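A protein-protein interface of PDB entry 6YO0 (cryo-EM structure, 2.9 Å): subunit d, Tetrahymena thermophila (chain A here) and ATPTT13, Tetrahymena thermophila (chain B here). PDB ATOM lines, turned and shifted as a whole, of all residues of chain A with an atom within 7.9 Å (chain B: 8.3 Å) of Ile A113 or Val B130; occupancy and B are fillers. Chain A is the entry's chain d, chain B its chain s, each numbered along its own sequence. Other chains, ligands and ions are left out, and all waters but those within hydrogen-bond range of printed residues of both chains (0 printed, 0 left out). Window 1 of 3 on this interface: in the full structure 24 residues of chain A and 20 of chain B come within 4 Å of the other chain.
Of the 14 printed residues of chain B, 7 touch a printed residue of chain A. Hydrophobic or aromatic side chains of chain B that line the printed part of chain A: Ile B124, Tyr B127, Ile B128, Val B130 and Ala B131. Among the printed residues, 10 pairs touch across the chains.
Printed residues of chain B within 4 Å of Tyr A108: Ala B131, Glu B134 and Asn B135. Asn A109 touches none of the printed residues of chain B. Ala A112 touches none of the printed residues of chain B. Of chain B, only Val B130 (3.6 Å) comes within 4 Å of Ile A113. No residue of chain B comes within 4 Å of Ser A114. Of the printed residues of chain B, Ala A120 touches Tyr B127 (2.8 Å). Printed residues of chain A within 4 Å of Ile B124: Tyr A67. Gly B126 touches none of the printed residues of chain A. Val B130 touches just one residue of chain A: Ile A113.
The backbone carbonyl oxygen (O) of Ile B124 is in hydrogen-bond range of the side-chain hydroxyl (OH) of Tyr A67. OH of Tyr B127 lies within hydrogen-bond range of O of Ala A120 (2.8 Å). OH of Tyr A67 lies close to N of Ile B128. The side-chain hydroxyl of Tyr A108 sits at hydrogen-bond distance from the side-chain amide oxygen of Asn B135.
The side-chain carboxylate (OE1) of Glu B134 lies within salt-bridge range of the guanidinium group (NH2) of Arg B137. O of Ala B131 lies close to ND2 of Asn B135 (3.0 Å). The side-chain hydroxyl of Ser A119 is in hydrogen-bond range of the backbone carbonyl oxygen of Gln A116 (2.9 Å).
Tyr A67 touches Tyr B127 (OH to C, 3.5 Å). CE1 of Tyr A108 touches CB of Ala B131 (3.6 Å). Glu B134 touches Tyr A108. Ile A113 touches Val B130. Gln A116 touches Tyr B127. Ile A117 touches Tyr B127 (CG2 to CE1, 3.2 Å).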
ATOM      1  N   TYR A  67     -26.456 -35.918 -10.425  1.00  0.00           N
ATOM      2  CA  TYR A  67     -25.897 -34.807 -11.187  1.00  0.00           C
ATOM      3  C   TYR A  67     -25.086 -35.296 -12.381  1.00  0.00           C
ATOM      4  O   TYR A  67     -25.139 -34.695 -13.459  1.00  0.00           O
ATOM      5  CB  TYR A  67     -25.044 -33.928 -10.272  1.00  0.00           C
ATOM      6  CG  TYR A  67     -25.835 -32.999  -9.370  1.00  0.00           C
ATOM      7  CD1 TYR A  67     -27.077 -32.506  -9.751  1.00  0.00           C
ATOM      8  CD2 TYR A  67     -25.340 -32.621  -8.133  1.00  0.00           C
ATOM      9  CE1 TYR A  67     -27.795 -31.664  -8.927  1.00  0.00           C
ATOM     10  CE2 TYR A  67     -26.053 -31.780  -7.305  1.00  0.00           C
ATOM     11  CZ  TYR A  67     -27.279 -31.303  -7.708  1.00  0.00           C
ATOM     12  OH  TYR A  67     -27.994 -30.464  -6.887  1.00  0.00           O
ATOM     13  N   TYR A 108     -28.805 -22.881 -21.472  1.00  0.00           N
ATOM     14  CA  TYR A 108     -28.399 -22.579 -20.108  1.00  0.00           C
ATOM     15  C   TYR A 108     -27.334 -21.490 -20.107  1.00  0.00           C
ATOM     16  O   TYR A 108     -26.588 -21.321 -21.075  1.00  0.00           O
ATOM     17  CB  TYR A 108     -27.849 -23.827 -19.414  1.00  0.00           C
ATOM     18  CG  TYR A 108     -28.824 -24.978 -19.245  1.00  0.00           C
ATOM     19  CD1 TYR A 108     -29.187 -25.420 -17.984  1.00  0.00           C
ATOM     20  CD2 TYR A 108     -29.344 -25.649 -20.342  1.00  0.00           C
ATOM     21  CE1 TYR A 108     -30.062 -26.476 -17.819  1.00  0.00           C
ATOM     22  CE2 TYR A 108     -30.218 -26.703 -20.187  1.00  0.00           C
ATOM     23  CZ  TYR A 108     -30.570 -27.116 -18.925  1.00  0.00           C
ATOM     24  OH  TYR A 108     -31.441 -28.169 -18.770  1.00  0.00           O
ATOM     25  N   ASN A 109     -27.283 -20.726 -19.021  1.00  0.00           N
ATOM     26  CA  ASN A 109     -26.237 -19.726 -18.812  1.00  0.00           C
ATOM     27  C   ASN A 109     -25.281 -20.261 -17.746  1.00  0.00           C
ATOM     28  O   ASN A 109     -25.377 -19.921 -16.568  1.00  0.00           O
ATOM     29  CB  ASN A 109     -26.846 -18.386 -18.405  1.00  0.00           C
ATOM     30  CG  ASN A 109     -27.824 -18.515 -17.255  1.00  0.00           C
ATOM     31  OD1 ASN A 109     -27.992 -19.594 -16.687  1.00  0.00           O
ATOM     32  ND2 ASN A 109     -28.469 -17.411 -16.901  1.00  0.00           N
ATOM     33  N   THR A 110     -24.327 -21.089 -18.180  1.00  0.00           N
ATOM     34  CA  THR A 110     -23.412 -21.711 -17.229  1.00  0.00           C
ATOM     35  C   THR A 110     -22.582 -20.677 -16.483  1.00  0.00           C
ATOM     36  O   THR A 110     -22.192 -20.906 -15.333  1.00  0.00           O
ATOM     37  CB  THR A 110     -22.473 -22.685 -17.942  1.00  0.00           C
ATOM     38  OG1 THR A 110     -21.802 -22.011 -19.013  1.00  0.00           O
ATOM     39  CG2 THR A 110     -23.246 -23.862 -18.498  1.00  0.00           C
ATOM     40  N   ASP A 111     -22.305 -19.536 -17.114  1.00  0.00           N
ATOM     41  CA  ASP A 111     -21.473 -18.526 -16.472  1.00  0.00           C
ATOM     42  C   ASP A 111     -22.112 -18.021 -15.185  1.00  0.00           C
ATOM     43  O   ASP A 111     -21.459 -17.962 -14.138  1.00  0.00           O
ATOM     44  CB  ASP A 111     -21.224 -17.369 -17.440  1.00  0.00           C
ATOM     45  CG  ASP A 111     -20.130 -16.433 -16.964  1.00  0.00           C
ATOM     46  OD1 ASP A 111     -19.908 -16.340 -15.739  1.00  0.00           O
ATOM     47  OD2 ASP A 111     -19.487 -15.789 -17.820  1.00  0.00           O
ATOM     48  N   ALA A 112     -23.401 -17.681 -15.233  1.00  0.00           N
ATOM     49  CA  ALA A 112     -24.045 -17.130 -14.047  1.00  0.00           C
ATOM     50  C   ALA A 112     -24.062 -18.140 -12.909  1.00  0.00           C
ATOM     51  O   ALA A 112     -23.758 -17.800 -11.760  1.00  0.00           O
ATOM     52  CB  ALA A 112     -25.468 -16.687 -14.387  1.00  0.00           C
ATOM     53  N   ILE A 113     -24.409 -19.389 -13.214  1.00  0.00           N
ATOM     54  CA  ILE A 113     -24.454 -20.430 -12.191  1.00  0.00           C
ATOM     55  C   ILE A 113     -23.069 -20.697 -11.619  1.00  0.00           C
ATOM     56  O   ILE A 113     -22.899 -20.840 -10.403  1.00  0.00           O
ATOM     57  CB  ILE A 113     -25.079 -21.716 -12.764  1.00  0.00           C
ATOM     58  CG1 ILE A 113     -26.591 -21.551 -12.961  1.00  0.00           C
ATOM     59  CG2 ILE A 113     -24.778 -22.899 -11.859  1.00  0.00           C
ATOM     60  CD1 ILE A 113     -26.991 -20.627 -14.084  1.00  0.00           C
ATOM     61  N   SER A 114     -22.056 -20.767 -12.484  1.00  0.00           N
ATOM     62  CA  SER A 114     -20.701 -21.043 -12.017  1.00  0.00           C
ATOM     63  C   SER A 114     -20.197 -19.988 -11.040  1.00  0.00           C
ATOM     64  O   SER A 114     -19.578 -20.322 -10.024  1.00  0.00           O
ATOM     65  CB  SER A 114     -19.757 -21.143 -13.211  1.00  0.00           C
ATOM     66  OG  SER A 114     -19.932 -20.048 -14.092  1.00  0.00           O
ATOM     67  N   LYS A 115     -20.431 -18.709 -11.330  1.00  0.00           N
ATOM     68  CA  LYS A 115     -19.943 -17.670 -10.428  1.00  0.00           C
ATOM     69  C   LYS A 115     -20.610 -17.751  -9.062  1.00  0.00           C
ATOM     70  O   LYS A 115     -19.937 -17.637  -8.031  1.00  0.00           O
ATOM     71  CB  LYS A 115     -20.138 -16.288 -11.049  1.00  0.00           C
ATOM     72  CG  LYS A 115     -19.497 -16.129 -12.423  1.00  0.00           C
ATOM     73  CD  LYS A 115     -18.057 -16.638 -12.460  1.00  0.00           C
ATOM     74  CE  LYS A 115     -17.156 -15.912 -11.477  1.00  0.00           C
ATOM     75  NZ  LYS A 115     -15.760 -16.434 -11.528  1.00  0.00           N
ATOM     76  N   GLN A 116     -21.929 -17.948  -9.024  1.00  0.00           N
ATOM     77  CA  GLN A 116     -22.608 -17.983  -7.733  1.00  0.00           C
ATOM     78  C   GLN A 116     -22.179 -19.194  -6.917  1.00  0.00           C
ATOM     79  O   GLN A 116     -22.052 -19.108  -5.690  1.00  0.00           O
ATOM     80  CB  GLN A 116     -24.123 -17.981  -7.928  1.00  0.00           C
ATOM     81  CG  GLN A 116     -24.635 -19.076  -8.856  1.00  0.00           C
ATOM     82  CD  GLN A 116     -26.152 -19.225  -8.852  1.00  0.00           C
ATOM     83  OE1 GLN A 116     -26.740 -19.635  -9.853  1.00  0.00           O
ATOM     84  NE2 GLN A 116     -26.789 -18.917  -7.726  1.00  0.00           N
ATOM     85  N   ILE A 117     -21.951 -20.331  -7.574  1.00  0.00           N
ATOM     86  CA  ILE A 117     -21.551 -21.520  -6.830  1.00  0.00           C
ATOM     87  C   ILE A 117     -20.085 -21.421  -6.426  1.00  0.00           C
ATOM     88  O   ILE A 117     -19.686 -21.962  -5.388  1.00  0.00           O
ATOM     89  CB  ILE A 117     -21.847 -22.802  -7.632  1.00  0.00           C
ATOM     90  CG1 ILE A 117     -21.090 -22.840  -8.960  1.00  0.00           C
ATOM     91  CG2 ILE A 117     -23.335 -22.917  -7.898  1.00  0.00           C
ATOM     92  CD1 ILE A 117     -19.681 -23.366  -8.856  1.00  0.00           C
ATOM     93  N   SER A 118     -19.261 -20.736  -7.225  1.00  0.00           N
ATOM     94  CA  SER A 118     -17.848 -20.602  -6.892  1.00  0.00           C
ATOM     95  C   SER A 118     -17.611 -19.462  -5.911  1.00  0.00           C
ATOM     96  O   SER A 118     -16.625 -19.486  -5.165  1.00  0.00           O
ATOM     97  CB  SER A 118     -17.021 -20.366  -8.158  1.00  0.00           C
ATOM     98  OG  SER A 118     -17.147 -21.438  -9.073  1.00  0.00           O
ATOM     99  N   SER A 119     -18.497 -18.467  -5.899  1.00  0.00           N
ATOM    100  CA  SER A 119     -18.305 -17.304  -5.040  1.00  0.00           C
ATOM    101  C   SER A 119     -18.488 -17.675  -3.574  1.00  0.00           C
ATOM    102  O   SER A 119     -17.566 -17.540  -2.762  1.00  0.00           O
ATOM    103  CB  SER A 119     -19.280 -16.198  -5.442  1.00  0.00           C
ATOM    104  OG  SER A 119     -20.620 -16.652  -5.360  1.00  0.00           O
ATOM    105  N   ALA A 120     -19.680 -18.145  -3.221  1.00  0.00           N
ATOM    106  CA  ALA A 120     -19.999 -18.507  -1.850  1.00  0.00           C
ATOM    107  C   ALA A 120     -21.046 -19.608  -1.869  1.00  0.00           C
ATOM    108  O   ALA A 120     -21.903 -19.651  -2.756  1.00  0.00           O
ATOM    109  CB  ALA A 120     -20.511 -17.303  -1.051  1.00  0.00           C
ATOM    110  N   ILE B 124     -24.616 -29.446  -1.382  1.00  0.00           N
ATOM    111  CA  ILE B 124     -24.844 -29.933  -2.739  1.00  0.00           C
ATOM    112  C   ILE B 124     -26.333 -29.938  -3.051  1.00  0.00           C
ATOM    113  O   ILE B 124     -26.747 -29.671  -4.185  1.00  0.00           O
ATOM    114  CB  ILE B 124     -24.213 -31.323  -2.927  1.00  0.00           C
ATOM    115  CG1 ILE B 124     -22.700 -31.268  -2.697  1.00  0.00           C
ATOM    116  CG2 ILE B 124     -24.488 -31.841  -4.316  1.00  0.00           C
ATOM    117  CD1 ILE B 124     -21.945 -30.363  -3.658  1.00  0.00           C
ATOM    118  N   CYS B 125     -27.162 -30.238  -2.051  1.00  0.00           N
ATOM    119  CA  CYS B 125     -28.598 -30.256  -2.286  1.00  0.00           C
ATOM    120  C   CYS B 125     -29.130 -28.846  -2.483  1.00  0.00           C
ATOM    121  O   CYS B 125     -30.108 -28.648  -3.209  1.00  0.00           O
ATOM    122  CB  CYS B 125     -29.311 -30.934  -1.120  1.00  0.00           C
ATOM    123  SG  CYS B 125     -31.103 -31.057  -1.314  1.00  0.00           S
ATOM    124  N   GLY B 126     -28.502 -27.858  -1.844  1.00  0.00           N
ATOM    125  CA  GLY B 126     -28.953 -26.487  -1.995  1.00  0.00           C
ATOM    126  C   GLY B 126     -28.985 -26.042  -3.444  1.00  0.00           C
ATOM    127  O   GLY B 126     -29.860 -25.266  -3.838  1.00  0.00           O
ATOM    128  N   TYR B 127     -28.041 -26.523  -4.254  1.00  0.00           N
ATOM    129  CA  TYR B 127     -27.892 -26.088  -5.635  1.00  0.00           C
ATOM    130  C   TYR B 127     -28.622 -26.995  -6.617  1.00  0.00           C
ATOM    131  O   TYR B 127     -28.333 -26.957  -7.819  1.00  0.00           O
ATOM    132  CB  TYR B 127     -26.408 -26.010  -6.001  1.00  0.00           C
ATOM    133  CG  TYR B 127     -25.665 -24.833  -5.398  1.00  0.00           C
ATOM    134  CD1 TYR B 127     -24.279 -24.829  -5.330  1.00  0.00           C
ATOM    135  CD2 TYR B 127     -26.346 -23.728  -4.895  1.00  0.00           C
ATOM    136  CE1 TYR B 127     -23.592 -23.759  -4.781  1.00  0.00           C
ATOM    137  CE2 TYR B 127     -25.667 -22.657  -4.347  1.00  0.00           C
ATOM    138  CZ  TYR B 127     -24.293 -22.677  -4.292  1.00  0.00           C
ATOM    139  OH  TYR B 127     -23.621 -21.607  -3.745  1.00  0.00           O
ATOM    140  N   ILE B 128     -29.554 -27.810  -6.135  1.00  0.00           N
ATOM    141  CA  ILE B 128     -30.432 -28.588  -6.999  1.00  0.00           C
ATOM    142  C   ILE B 128     -31.524 -27.649  -7.494  1.00  0.00           C
ATOM    143  O   ILE B 128     -31.664 -26.532  -6.987  1.00  0.00           O
ATOM    144  CB  ILE B 128     -31.014 -29.795  -6.241  1.00  0.00           C
ATOM    145  CG1 ILE B 128     -31.688 -30.783  -7.192  1.00  0.00           C
ATOM    146  CG2 ILE B 128     -32.030 -29.325  -5.221  1.00  0.00           C
ATOM    147  CD1 ILE B 128     -32.280 -31.976  -6.483  1.00  0.00           C
ATOM    148  N   ASP B 129     -32.296 -28.083  -8.488  1.00  0.00           N
ATOM    149  CA  ASP B 129     -33.441 -27.368  -9.043  1.00  0.00           C
ATOM    150  C   ASP B 129     -33.018 -26.274 -10.013  1.00  0.00           C
ATOM    151  O   ASP B 129     -33.890 -25.629 -10.607  1.00  0.00           O
ATOM    152  CB  ASP B 129     -34.312 -26.738  -7.943  1.00  0.00           C
ATOM    153  CG  ASP B 129     -35.649 -26.240  -8.456  1.00  0.00           C
ATOM    154  OD1 ASP B 129     -36.030 -26.592  -9.589  1.00  0.00           O
ATOM    155  OD2 ASP B 129     -36.324 -25.494  -7.716  1.00  0.00           O
ATOM    156  N   VAL B 130     -31.721 -26.042 -10.203  1.00  0.00           N
ATOM    157  CA  VAL B 130     -31.289 -24.987 -11.116  1.00  0.00           C
ATOM    158  C   VAL B 130     -31.738 -25.301 -12.538  1.00  0.00           C
ATOM    159  O   VAL B 130     -32.425 -24.502 -13.185  1.00  0.00           O
ATOM    160  CB  VAL B 130     -29.763 -24.792 -11.040  1.00  0.00           C
ATOM    161  CG1 VAL B 130     -29.013 -26.111 -11.236  1.00  0.00           C
ATOM    162  CG2 VAL B 130     -29.313 -23.780 -12.074  1.00  0.00           C
ATOM    163  N   ALA B 131     -31.357 -26.475 -13.044  1.00  0.00           N
ATOM    164  CA  ALA B 131     -31.752 -26.856 -14.394  1.00  0.00           C
ATOM    165  C   ALA B 131     -33.262 -26.951 -14.546  1.00  0.00           C
ATOM    166  O   ALA B 131     -33.798 -26.627 -15.612  1.00  0.00           O
ATOM    167  CB  ALA B 131     -31.101 -28.183 -14.772  1.00  0.00           C
ATOM    168  N   ASN B 132     -33.971 -27.383 -13.501  1.00  0.00           N
ATOM    169  CA  ASN B 132     -35.424 -27.457 -13.593  1.00  0.00           C
ATOM    170  C   ASN B 132     -36.032 -26.073 -13.766  1.00  0.00           C
ATOM    171  O   ASN B 132     -36.937 -25.882 -14.585  1.00  0.00           O
ATOM    172  CB  ASN B 132     -35.991 -28.145 -12.355  1.00  0.00           C
ATOM    173  CG  ASN B 132     -37.505 -28.151 -12.334  1.00  0.00           C
ATOM    174  OD1 ASN B 132     -38.142 -28.945 -13.025  1.00  0.00           O
ATOM    175  ND2 ASN B 132     -38.090 -27.258 -11.546  1.00  0.00           N
ATOM    176  N   LYS B 133     -35.539 -25.091 -13.010  1.00  0.00           N
ATOM    177  CA  LYS B 133     -36.036 -23.729 -13.161  1.00  0.00           C
ATOM    178  C   LYS B 133     -35.669 -23.170 -14.528  1.00  0.00           C
ATOM    179  O   LYS B 133     -36.470 -22.468 -15.157  1.00  0.00           O
ATOM    180  CB  LYS B 133     -35.484 -22.840 -12.051  1.00  0.00           C
ATOM    181  CG  LYS B 133     -35.951 -21.404 -12.139  1.00  0.00           C
ATOM    182  CD  LYS B 133     -35.417 -20.574 -10.991  1.00  0.00           C
ATOM    183  CE  LYS B 133     -35.899 -19.137 -11.085  1.00  0.00           C
ATOM    184  NZ  LYS B 133     -35.469 -18.482 -12.350  1.00  0.00           N
ATOM    185  N   GLU B 134     -34.460 -23.474 -15.001  1.00  0.00           N
ATOM    186  CA  GLU B 134     -34.054 -23.062 -16.340  1.00  0.00           C
ATOM    187  C   GLU B 134     -35.023 -23.594 -17.383  1.00  0.00           C
ATOM    188  O   GLU B 134     -35.467 -22.858 -18.271  1.00  0.00           O
ATOM    189  CB  GLU B 134     -32.634 -23.555 -16.620  1.00  0.00           C
ATOM    190  CG  GLU B 134     -32.102 -23.205 -17.998  1.00  0.00           C
ATOM    191  CD  GLU B 134     -31.764 -21.740 -18.132  1.00  0.00           C
ATOM    192  OE1 GLU B 134     -31.940 -20.996 -17.143  1.00  0.00           O
ATOM    193  OE2 GLU B 134     -31.327 -21.323 -19.225  1.00  0.00           O
ATOM    194  N   ASN B 135     -35.373 -24.876 -17.283  1.00  0.00           N
ATOM    195  CA  ASN B 135     -36.311 -25.458 -18.234  1.00  0.00           C
ATOM    196  C   ASN B 135     -37.667 -24.773 -18.148  1.00  0.00           C
ATOM    197  O   ASN B 135     -38.314 -24.533 -19.173  1.00  0.00           O
ATOM    198  CB  ASN B 135     -36.445 -26.957 -17.982  1.00  0.00           C
ATOM    199  CG  ASN B 135     -35.106 -27.666 -17.975  1.00  0.00           C
ATOM    200  OD1 ASN B 135     -34.146 -27.209 -18.597  1.00  0.00           O
ATOM    201  ND2 ASN B 135     -35.033 -28.791 -17.275  1.00  0.00           N
ATOM    202  N   VAL B 136     -38.112 -24.443 -16.935  1.00  0.00           N
ATOM    203  CA  VAL B 136     -39.397 -23.767 -16.781  1.00  0.00           C
ATOM    204  C   VAL B 136     -39.417 -22.485 -17.601  1.00  0.00           C
ATOM    205  O   VAL B 136     -40.354 -22.228 -18.366  1.00  0.00           O
ATOM    206  CB  VAL B 136     -39.683 -23.484 -15.296  1.00  0.00           C
ATOM    207  CG1 VAL B 136     -40.913 -22.611 -15.156  1.00  0.00           C
ATOM    208  CG2 VAL B 136     -39.873 -24.777 -14.535  1.00  0.00           C
ATOM    209  N   ARG B 137     -38.380 -21.660 -17.454  1.00  0.00           N
ATOM    210  CA  ARG B 137     -38.316 -20.417 -18.214  1.00  0.00           C
ATOM    211  C   ARG B 137     -38.277 -20.691 -19.712  1.00  0.00           C
ATOM    212  O   ARG B 137     -39.078 -20.141 -20.477  1.00  0.00           O
ATOM    213  CB  ARG B 137     -37.095 -19.606 -17.785  1.00  0.00           C
ATOM    214  CG  ARG B 137     -36.858 -18.369 -18.628  1.00  0.00           C
ATOM    215  CD  ARG B 137     -35.682 -17.558 -18.119  1.00  0.00           C
ATOM    216  NE  ARG B 137     -34.435 -18.314 -18.138  1.00  0.00           N
ATOM    217  CZ  ARG B 137     -33.306 -17.902 -17.572  1.00  0.00           C
ATOM    218  NH1 ARG B 137     -33.261 -16.742 -16.933  1.00  0.00           N
ATOM    219  NH2 ARG B 137     -32.218 -18.652 -17.642  1.00  0.00           N
